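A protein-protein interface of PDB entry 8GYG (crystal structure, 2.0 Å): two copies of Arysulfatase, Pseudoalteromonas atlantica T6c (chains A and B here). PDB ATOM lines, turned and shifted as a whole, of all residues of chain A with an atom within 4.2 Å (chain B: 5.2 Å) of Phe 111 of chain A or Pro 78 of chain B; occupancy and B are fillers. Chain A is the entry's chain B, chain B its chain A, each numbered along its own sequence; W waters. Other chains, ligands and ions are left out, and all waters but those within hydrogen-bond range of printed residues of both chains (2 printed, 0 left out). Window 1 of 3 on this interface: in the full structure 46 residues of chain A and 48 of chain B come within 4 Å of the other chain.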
ATOM      1  N   PRO A  78      17.822   3.697  -4.384  1.00  0.00           N
ATOM      2  CA  PRO A  78      17.562   5.104  -4.721  1.00  0.00           C
ATOM      3  C   PRO A  78      17.812   5.405  -6.186  1.00  0.00           C
ATOM      4  O   PRO A  78      17.007   6.114  -6.804  1.00  0.00           O
ATOM      5  CB  PRO A  78      18.534   5.867  -3.815  1.00  0.00           C
ATOM      6  CG  PRO A  78      18.740   4.985  -2.666  1.00  0.00           C
ATOM      7  CD  PRO A  78      18.704   3.588  -3.203  1.00  0.00           C
ATOM      8  N   GLY A 107      12.195   7.668   2.544  1.00  0.00           N
ATOM      9  CA  GLY A 107      13.411   8.460   2.500  1.00  0.00           C
ATOM     10  C   GLY A 107      13.948   8.643   1.095  1.00  0.00           C
ATOM     11  O   GLY A 107      14.483   9.702   0.763  1.00  0.00           O
ATOM     12  N   ILE A 108      13.818   7.611   0.248  1.00  0.00           N
ATOM     13  CA  ILE A 108      14.181   7.747  -1.164  1.00  0.00           C
ATOM     14  C   ILE A 108      13.368   8.859  -1.823  1.00  0.00           C
ATOM     15  O   ILE A 108      13.921   9.716  -2.525  1.00  0.00           O
ATOM     16  CB  ILE A 108      14.001   6.409  -1.908  1.00  0.00           C
ATOM     17  CG1 ILE A 108      15.079   5.396  -1.513  1.00  0.00           C
ATOM     18  CG2 ILE A 108      14.075   6.649  -3.405  1.00  0.00           C
ATOM     19  CD1 ILE A 108      14.954   4.034  -2.252  1.00  0.00           C
ATOM     20  N   PHE A 109      12.042   8.861  -1.608  1.00  0.00           N
ATOM     21  CA  PHE A 109      11.210   9.924  -2.176  1.00  0.00           C
ATOM     22  C   PHE A 109      11.587  11.296  -1.617  1.00  0.00           C
ATOM     23  O   PHE A 109      11.497  12.301  -2.334  1.00  0.00           O
ATOM     24  CB  PHE A 109       9.727   9.657  -1.921  1.00  0.00           C
ATOM     25  CG  PHE A 109       9.215   8.383  -2.509  1.00  0.00           C
ATOM     26  CD1 PHE A 109       9.678   7.908  -3.724  1.00  0.00           C
ATOM     27  CD2 PHE A 109       8.250   7.649  -1.828  1.00  0.00           C
ATOM     28  CE1 PHE A 109       9.177   6.725  -4.265  1.00  0.00           C
ATOM     29  CE2 PHE A 109       7.746   6.460  -2.359  1.00  0.00           C
ATOM     30  CZ  PHE A 109       8.213   5.999  -3.572  1.00  0.00           C
ATOM     31  N   ALA A 110      12.018  11.360  -0.348  1.00  0.00           N
ATOM     32  CA  ALA A 110      12.498  12.622   0.216  1.00  0.00           C
ATOM     33  C   ALA A 110      13.838  13.033  -0.387  1.00  0.00           C
ATOM     34  O   ALA A 110      14.111  14.232  -0.536  1.00  0.00           O
ATOM     35  CB  ALA A 110      12.626  12.511   1.730  1.00  0.00           C
ATOM     36  N   PHE A 111      14.692  12.059  -0.712  1.00  0.00           N
ATOM     37  CA  PHE A 111      15.947  12.372  -1.391  1.00  0.00           C
ATOM     38  C   PHE A 111      15.683  12.923  -2.785  1.00  0.00           C
ATOM     39  O   PHE A 111      16.438  13.773  -3.270  1.00  0.00           O
ATOM     40  CB  PHE A 111      16.838  11.124  -1.455  1.00  0.00           C
ATOM     41  CG  PHE A 111      17.714  11.042  -2.697  1.00  0.00           C
ATOM     42  CD1 PHE A 111      18.913  11.745  -2.765  1.00  0.00           C
ATOM     43  CD2 PHE A 111      17.343  10.250  -3.789  1.00  0.00           C
ATOM     44  CE1 PHE A 111      19.734  11.665  -3.900  1.00  0.00           C
ATOM     45  CE2 PHE A 111      18.147  10.167  -4.928  1.00  0.00           C
ATOM     46  CZ  PHE A 111      19.350  10.880  -4.979  1.00  0.00           C
ATOM     47  N   MET A 112      14.581  12.497  -3.406  1.00  0.00           N
ATOM     48  CA  MET A 112      14.214  12.909  -4.758  1.00  0.00           C
ATOM     49  C   MET A 112      13.513  14.260  -4.829  1.00  0.00           C
ATOM     50  O   MET A 112      13.399  14.802  -5.934  1.00  0.00           O
ATOM     51  CB  MET A 112      13.280  11.880  -5.393  1.00  0.00           C
ATOM     52  CG  MET A 112      13.979  10.610  -5.841  1.00  0.00           C
ATOM     53  SD  MET A 112      12.805   9.291  -6.147  1.00  0.00           S
ATOM     54  CE  MET A 112      11.931   9.911  -7.599  1.00  0.00           C
ATOM     55  N   LYS A 113      13.036  14.804  -3.704  1.00  0.00           N
ATOM     56  CA  LYS A 113      11.969  15.798  -3.757  1.00  0.00           C
ATOM     57  C   LYS A 113      12.390  17.026  -4.547  1.00  0.00           C
ATOM     58  O   LYS A 113      11.674  17.469  -5.451  1.00  0.00           O
ATOM     59  CB  LYS A 113      11.529  16.197  -2.343  1.00  0.00           C
ATOM     60  CG  LYS A 113      10.124  16.842  -2.315  1.00  0.00           C
ATOM     61  CD  LYS A 113       9.618  17.088  -0.897  1.00  0.00           C
ATOM     62  CE  LYS A 113       8.313  17.865  -0.930  1.00  0.00           C
ATOM     63  NZ  LYS A 113       8.406  18.970  -1.927  1.00  0.00           N
ATOM     64  N   PHE B  71      19.058  13.214 -11.556  1.00  0.00           N
ATOM     65  CA  PHE B  71      19.424  11.982 -10.866  1.00  0.00           C
ATOM     66  C   PHE B  71      20.483  11.189 -11.610  1.00  0.00           C
ATOM     67  O   PHE B  71      21.124  10.319 -11.004  1.00  0.00           O
ATOM     68  CB  PHE B  71      18.177  11.135 -10.620  1.00  0.00           C
ATOM     69  CG  PHE B  71      17.169  11.831  -9.784  1.00  0.00           C
ATOM     70  CD1 PHE B  71      17.489  12.206  -8.495  1.00  0.00           C
ATOM     71  CD2 PHE B  71      15.927  12.174 -10.296  1.00  0.00           C
ATOM     72  CE1 PHE B  71      16.592  12.893  -7.708  1.00  0.00           C
ATOM     73  CE2 PHE B  71      15.014  12.853  -9.505  1.00  0.00           C
ATOM     74  CZ  PHE B  71      15.352  13.210  -8.209  1.00  0.00           C
ATOM     75  N   THR B  74      23.151  12.504  -9.418  1.00  0.00           N
ATOM     76  CA  THR B  74      23.103  12.225  -7.987  1.00  0.00           C
ATOM     77  C   THR B  74      22.656  10.808  -7.632  1.00  0.00           C
ATOM     78  O   THR B  74      22.628  10.482  -6.442  1.00  0.00           O
ATOM     79  CB  THR B  74      22.158  13.191  -7.273  1.00  0.00           C
ATOM     80  OG1 THR B  74      20.819  12.950  -7.731  1.00  0.00           O
ATOM     81  CG2 THR B  74      22.561  14.677  -7.506  1.00  0.00           C
ATOM     82  N   GLY B  75      22.309   9.964  -8.610  1.00  0.00           N
ATOM     83  CA  GLY B  75      21.769   8.640  -8.309  1.00  0.00           C
ATOM     84  C   GLY B  75      22.630   7.784  -7.393  1.00  0.00           C
ATOM     85  O   GLY B  75      22.106   6.952  -6.630  1.00  0.00           O
ATOM     86  N   GLY B  76      23.940   7.964  -7.436  1.00  0.00           N
ATOM     87  CA  GLY B  76      24.832   7.149  -6.642  1.00  0.00           C
ATOM     88  C   GLY B  76      25.250   7.766  -5.340  1.00  0.00           C
ATOM     89  O   GLY B  76      25.972   7.122  -4.568  1.00  0.00           O
ATOM     90  N   LEU B  77      24.809   8.989  -5.057  1.00  0.00           N
ATOM     91  CA  LEU B  77      25.152   9.605  -3.783  1.00  0.00           C
ATOM     92  C   LEU B  77      24.573   8.849  -2.597  1.00  0.00           C
ATOM     93  O   LEU B  77      25.282   8.724  -1.580  1.00  0.00           O
ATOM     94  CB  LEU B  77      24.721  11.082  -3.795  1.00  0.00           C
ATOM     95  CG  LEU B  77      25.198  11.971  -2.635  1.00  0.00           C
ATOM     96  CD1 LEU B  77      26.665  11.768  -2.310  1.00  0.00           C
ATOM     97  CD2 LEU B  77      24.916  13.438  -2.944  1.00  0.00           C
ATOM     98  N   PRO B  78      23.346   8.328  -2.630  1.00  0.00           N
ATOM     99  CA  PRO B  78      22.896   7.547  -1.474  1.00  0.00           C
ATOM    100  C   PRO B  78      23.743   6.319  -1.221  1.00  0.00           C
ATOM    101  O   PRO B  78      23.913   5.936  -0.055  1.00  0.00           O
ATOM    102  CB  PRO B  78      21.455   7.204  -1.829  1.00  0.00           C
ATOM    103  CG  PRO B  78      21.031   8.330  -2.703  1.00  0.00           C
ATOM    104  CD  PRO B  78      22.222   8.603  -3.557  1.00  0.00           C
ATOM    105  N   ALA B  79      24.308   5.705  -2.263  1.00  0.00           N
ATOM    106  CA  ALA B  79      25.172   4.549  -2.053  1.00  0.00           C
ATOM    107  C   ALA B  79      26.469   4.973  -1.392  1.00  0.00           C
ATOM    108  O   ALA B  79      26.899   4.374  -0.403  1.00  0.00           O
ATOM    109  CB  ALA B  79      25.454   3.834  -3.375  1.00  0.00           C
ATOM    110  N   LEU B  80      27.086   6.033  -1.913  1.00  0.00           N
ATOM    111  CA  LEU B  80      28.360   6.495  -1.377  1.00  0.00           C
ATOM    112  C   LEU B  80      28.267   6.815   0.109  1.00  0.00           C
ATOM    113  O   LEU B  80      29.126   6.403   0.902  1.00  0.00           O
ATOM    114  CB  LEU B  80      28.829   7.714  -2.170  1.00  0.00           C
ATOM    115  CG  LEU B  80      30.159   8.341  -1.765  1.00  0.00           C
ATOM    116  CD1 LEU B  80      31.296   7.311  -1.785  1.00  0.00           C
ATOM    117  CD2 LEU B  80      30.441   9.461  -2.720  1.00  0.00           C
ATOM    118  N   LEU B  81      27.232   7.553   0.514  1.00  0.00           N
ATOM    119  CA  LEU B  81      27.149   7.924   1.920  1.00  0.00           C
ATOM    120  C   LEU B  81      26.816   6.722   2.800  1.00  0.00           C
ATOM    121  O   LEU B  81      27.415   6.543   3.871  1.00  0.00           O
ATOM    122  CB  LEU B  81      26.118   9.035   2.122  1.00  0.00           C
ATOM    123  CG  LEU B  81      26.365  10.338   1.348  1.00  0.00           C
ATOM    124  CD1 LEU B  81      25.540  11.479   1.971  1.00  0.00           C
ATOM    125  CD2 LEU B  81      27.846  10.696   1.276  1.00  0.00           C
ATOM    126  N   SER B  82      25.855   5.895   2.386  1.00  0.00           N
ATOM    127  CA  SER B  82      25.438   4.818   3.272  1.00  0.00           C
ATOM    128  C   SER B  82      26.527   3.760   3.404  1.00  0.00           C
ATOM    129  O   SER B  82      26.703   3.186   4.485  1.00  0.00           O
ATOM    130  CB  SER B  82      24.118   4.196   2.792  1.00  0.00           C
ATOM    131  OG  SER B  82      24.198   3.709   1.471  1.00  0.00           O
ATOM    132  N   LEU B  83      27.282   3.499   2.327  1.00  0.00           N
ATOM    133  CA  LEU B  83      28.300   2.452   2.395  1.00  0.00           C
ATOM    134  C   LEU B  83      29.496   2.903   3.215  1.00  0.00           C
ATOM    135  O   LEU B  83      30.082   2.104   3.959  1.00  0.00           O
ATOM    136  CB  LEU B  83      28.737   2.030   0.988  1.00  0.00           C
ATOM    137  CG  LEU B  83      27.763   1.178   0.183  1.00  0.00           C
ATOM    138  CD1 LEU B  83      28.326   0.948  -1.211  1.00  0.00           C
ATOM    139  CD2 LEU B  83      27.495  -0.148   0.904  1.00  0.00           C
ATOM    140  N   GLU B 103      18.523  19.607   1.453  1.00  0.00           N
ATOM    141  CA  GLU B 103      17.307  18.803   1.526  1.00  0.00           C
ATOM    142  C   GLU B 103      17.520  17.433   0.902  1.00  0.00           C
ATOM    143  O   GLU B 103      16.985  16.431   1.392  1.00  0.00           O
ATOM    144  CB  GLU B 103      16.151  19.527   0.823  1.00  0.00           C
ATOM    145  CG  GLU B 103      15.646  20.771   1.558  1.00  0.00           C
ATOM    146  CD  GLU B 103      16.324  22.078   1.103  1.00  0.00           C
ATOM    147  OE1 GLU B 103      17.495  22.041   0.645  1.00  0.00           O
ATOM    148  OE2 GLU B 103      15.679  23.151   1.219  1.00  0.00           O
ATOM    149  N   THR B 104      18.297  17.382  -0.181  1.00  0.00           N
ATOM    150  CA  THR B 104      18.585  16.131  -0.878  1.00  0.00           C
ATOM    151  C   THR B 104      19.396  15.186   0.008  1.00  0.00           C
ATOM    152  O   THR B 104      19.046  14.007   0.163  1.00  0.00           O
ATOM    153  CB  THR B 104      19.333  16.443  -2.182  1.00  0.00           C
ATOM    154  OG1 THR B 104      18.511  17.274  -3.032  1.00  0.00           O
ATOM    155  CG2 THR B 104      19.723  15.163  -2.921  1.00  0.00           C
ATOM    156  N   GLY B 107      17.443  13.773   2.850  1.00  0.00           N
ATOM    157  CA  GLY B 107      16.659  12.619   2.432  1.00  0.00           C
ATOM    158  C   GLY B 107      17.456  11.323   2.439  1.00  0.00           C
ATOM    159  O   GLY B 107      16.916  10.256   2.739  1.00  0.00           O
ATOM    160  N   ILE B 108      18.744  11.396   2.090  1.00  0.00           N
ATOM    161  CA  ILE B 108      19.613  10.222   2.176  1.00  0.00           C
ATOM    162  C   ILE B 108      19.694   9.715   3.614  1.00  0.00           C
ATOM    163  O   ILE B 108      19.623   8.502   3.875  1.00  0.00           O
ATOM    164  CB  ILE B 108      21.008  10.557   1.619  1.00  0.00           C
ATOM    165  CG1 ILE B 108      20.930  10.755   0.094  1.00  0.00           C
ATOM    166  CG2 ILE B 108      22.009   9.466   2.006  1.00  0.00           C
ATOM    167  CD1 ILE B 108      22.191  11.327  -0.516  1.00  0.00           C
ATOM    168  N   PHE B 111      16.609   7.884   4.222  1.00  0.00           N
ATOM    169  CA  PHE B 111      16.657   6.561   3.602  1.00  0.00           C
ATOM    170  C   PHE B 111      17.470   5.608   4.462  1.00  0.00           C
ATOM    171  O   PHE B 111      17.114   4.436   4.623  1.00  0.00           O
ATOM    172  CB  PHE B 111      17.227   6.691   2.180  1.00  0.00           C
ATOM    173  CG  PHE B 111      17.936   5.463   1.665  1.00  0.00           C
ATOM    174  CD1 PHE B 111      17.223   4.380   1.163  1.00  0.00           C
ATOM    175  CD2 PHE B 111      19.319   5.421   1.645  1.00  0.00           C
ATOM    176  CE1 PHE B 111      17.900   3.245   0.676  1.00  0.00           C
ATOM    177  CE2 PHE B 111      20.007   4.318   1.167  1.00  0.00           C
ATOM    178  CZ  PHE B 111      19.313   3.226   0.679  1.00  0.00           C
HETATM  179  O   HOH W   1      16.749  16.005  -4.961  1.00  0.00           O
HETATM  180  O   HOH W   2      15.287  16.622  -2.012  1.00  0.00           O
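OG of Ser 82 of chain B is in hydrogen-bond range of O of Pro 78 of chain B, 2.7 Å away.
The backbone carbonyl oxygen of Gly 107 of chain B sits close to the backbone carbonyl oxygen of Gly 107 of chain A, 3.2 Å away.
Pro 78 of chain B touches its own counterpart, Pro 78 of chain A.
Pro 78 of chain A touches Phe 111 of chain B, and with the chains exchanged Phe 111 of chain A touches Pro 78 of chain B.
Gly 107 of chain A touches its own counterpart, Gly 107 of chain B.
Gly 107 of chain A touches Phe 111 of chain B, and with the chains exchanged Phe 111 of chain A touches Gly 107 of chain B.
Along chain A the printed residues that touch a printed residue of chain B span positions 78 to 112.
Of the 16 printed residues of chain B, 7 touch a printed residue of chain A.
Hydrophobic or aromatic side chains of chain B that line the printed part of chain A: Phe 71, Pro 78, Ile 108 and Phe 111.
Among the printed residues, no Asp or Glu carboxylate lies within 4 Å of a Lys or Arg side-chain nitrogen of the other chain.
Pro 78 of chain B touches Pro 78 of chain A.
Phe 111 of chain B touches Pro 78 of chain A.
CA of Gly 107 of chain A touches N of Phe 111 of chain B, 3.7 Å away.
Phe 111 of chain B touches Ile 108 of chain A.
O of Thr 74 of chain B touches CZ of Phe 111 of chain A, at 3.6 Å.
CE1 of Phe 111 of chain A touches CG of Pro 78 of chain B (3.8 Å).
Phe 111 of chain A touches Thr 104 of chain B (CD1 to CG2, 3.5 Å).
Phe 111 of chain A touches Gly 107 of chain B.
Ile 108 of chain B touches Phe 111 of chain A (CG1 to CD1, 3.6 Å).
Phe 71 of chain B touches Met 112 of chain A (CZ to O, 3.4 Å).
Phe 111 of chain A touches just these residues of chain B: Thr 74, Pro 78, Thr 104, Gly 107 and Ile 108.
Of chain A, only Pro 78 (3.6 Å) and Phe 111 (3.8 Å) come within 4 Å of Pro 78 of chain B.
Of the printed residues of chain A, Phe 71 of chain B touches Met 112.
Of the printed residues of chain A, Gly 107 of chain B touches Gly 107 (3.2 Å) and Phe 111 (3.8 Å).
Of the printed residues of chain A, Phe 111 of chain B touches Pro 78, Gly 107 and Ile 108.
Of the printed residues of chain B, Ile 108 of chain A touches Phe 111 (3.6 Å).
Of the printed residues of chain A, Thr 104 of chain B touches Phe 111 (3.5 Å).
Gly 75 of chain B touches none of the printed residues of chain A.
The nearest residue of chain B that does not touch Phe 111 of chain A is Phe 71 of chain B (4.2 Å).
The nearest printed residue of chain A that does not touch Pro 78 of chain B is Ile 108 of chain A (6.6 Å).
The nearest printed residue of chain A that does not touch Thr 74 of chain B is Pro 78 of chain A (6.7 Å).
Water W1 lies within hydrogen-bond range of O of Phe 111 of chain A (2.8 Å) and OG1 of Thr 104 of chain B (2.9 Å).
Water W2 lies within hydrogen-bond range of the backbone carbonyl oxygen of Ala 110 of chain A, the backbone carbonyl oxygen of Phe 111 of chain A, the backbone NH of Lys 113 of chain A and the side-chain hydroxyl of Thr 104 of chain B.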
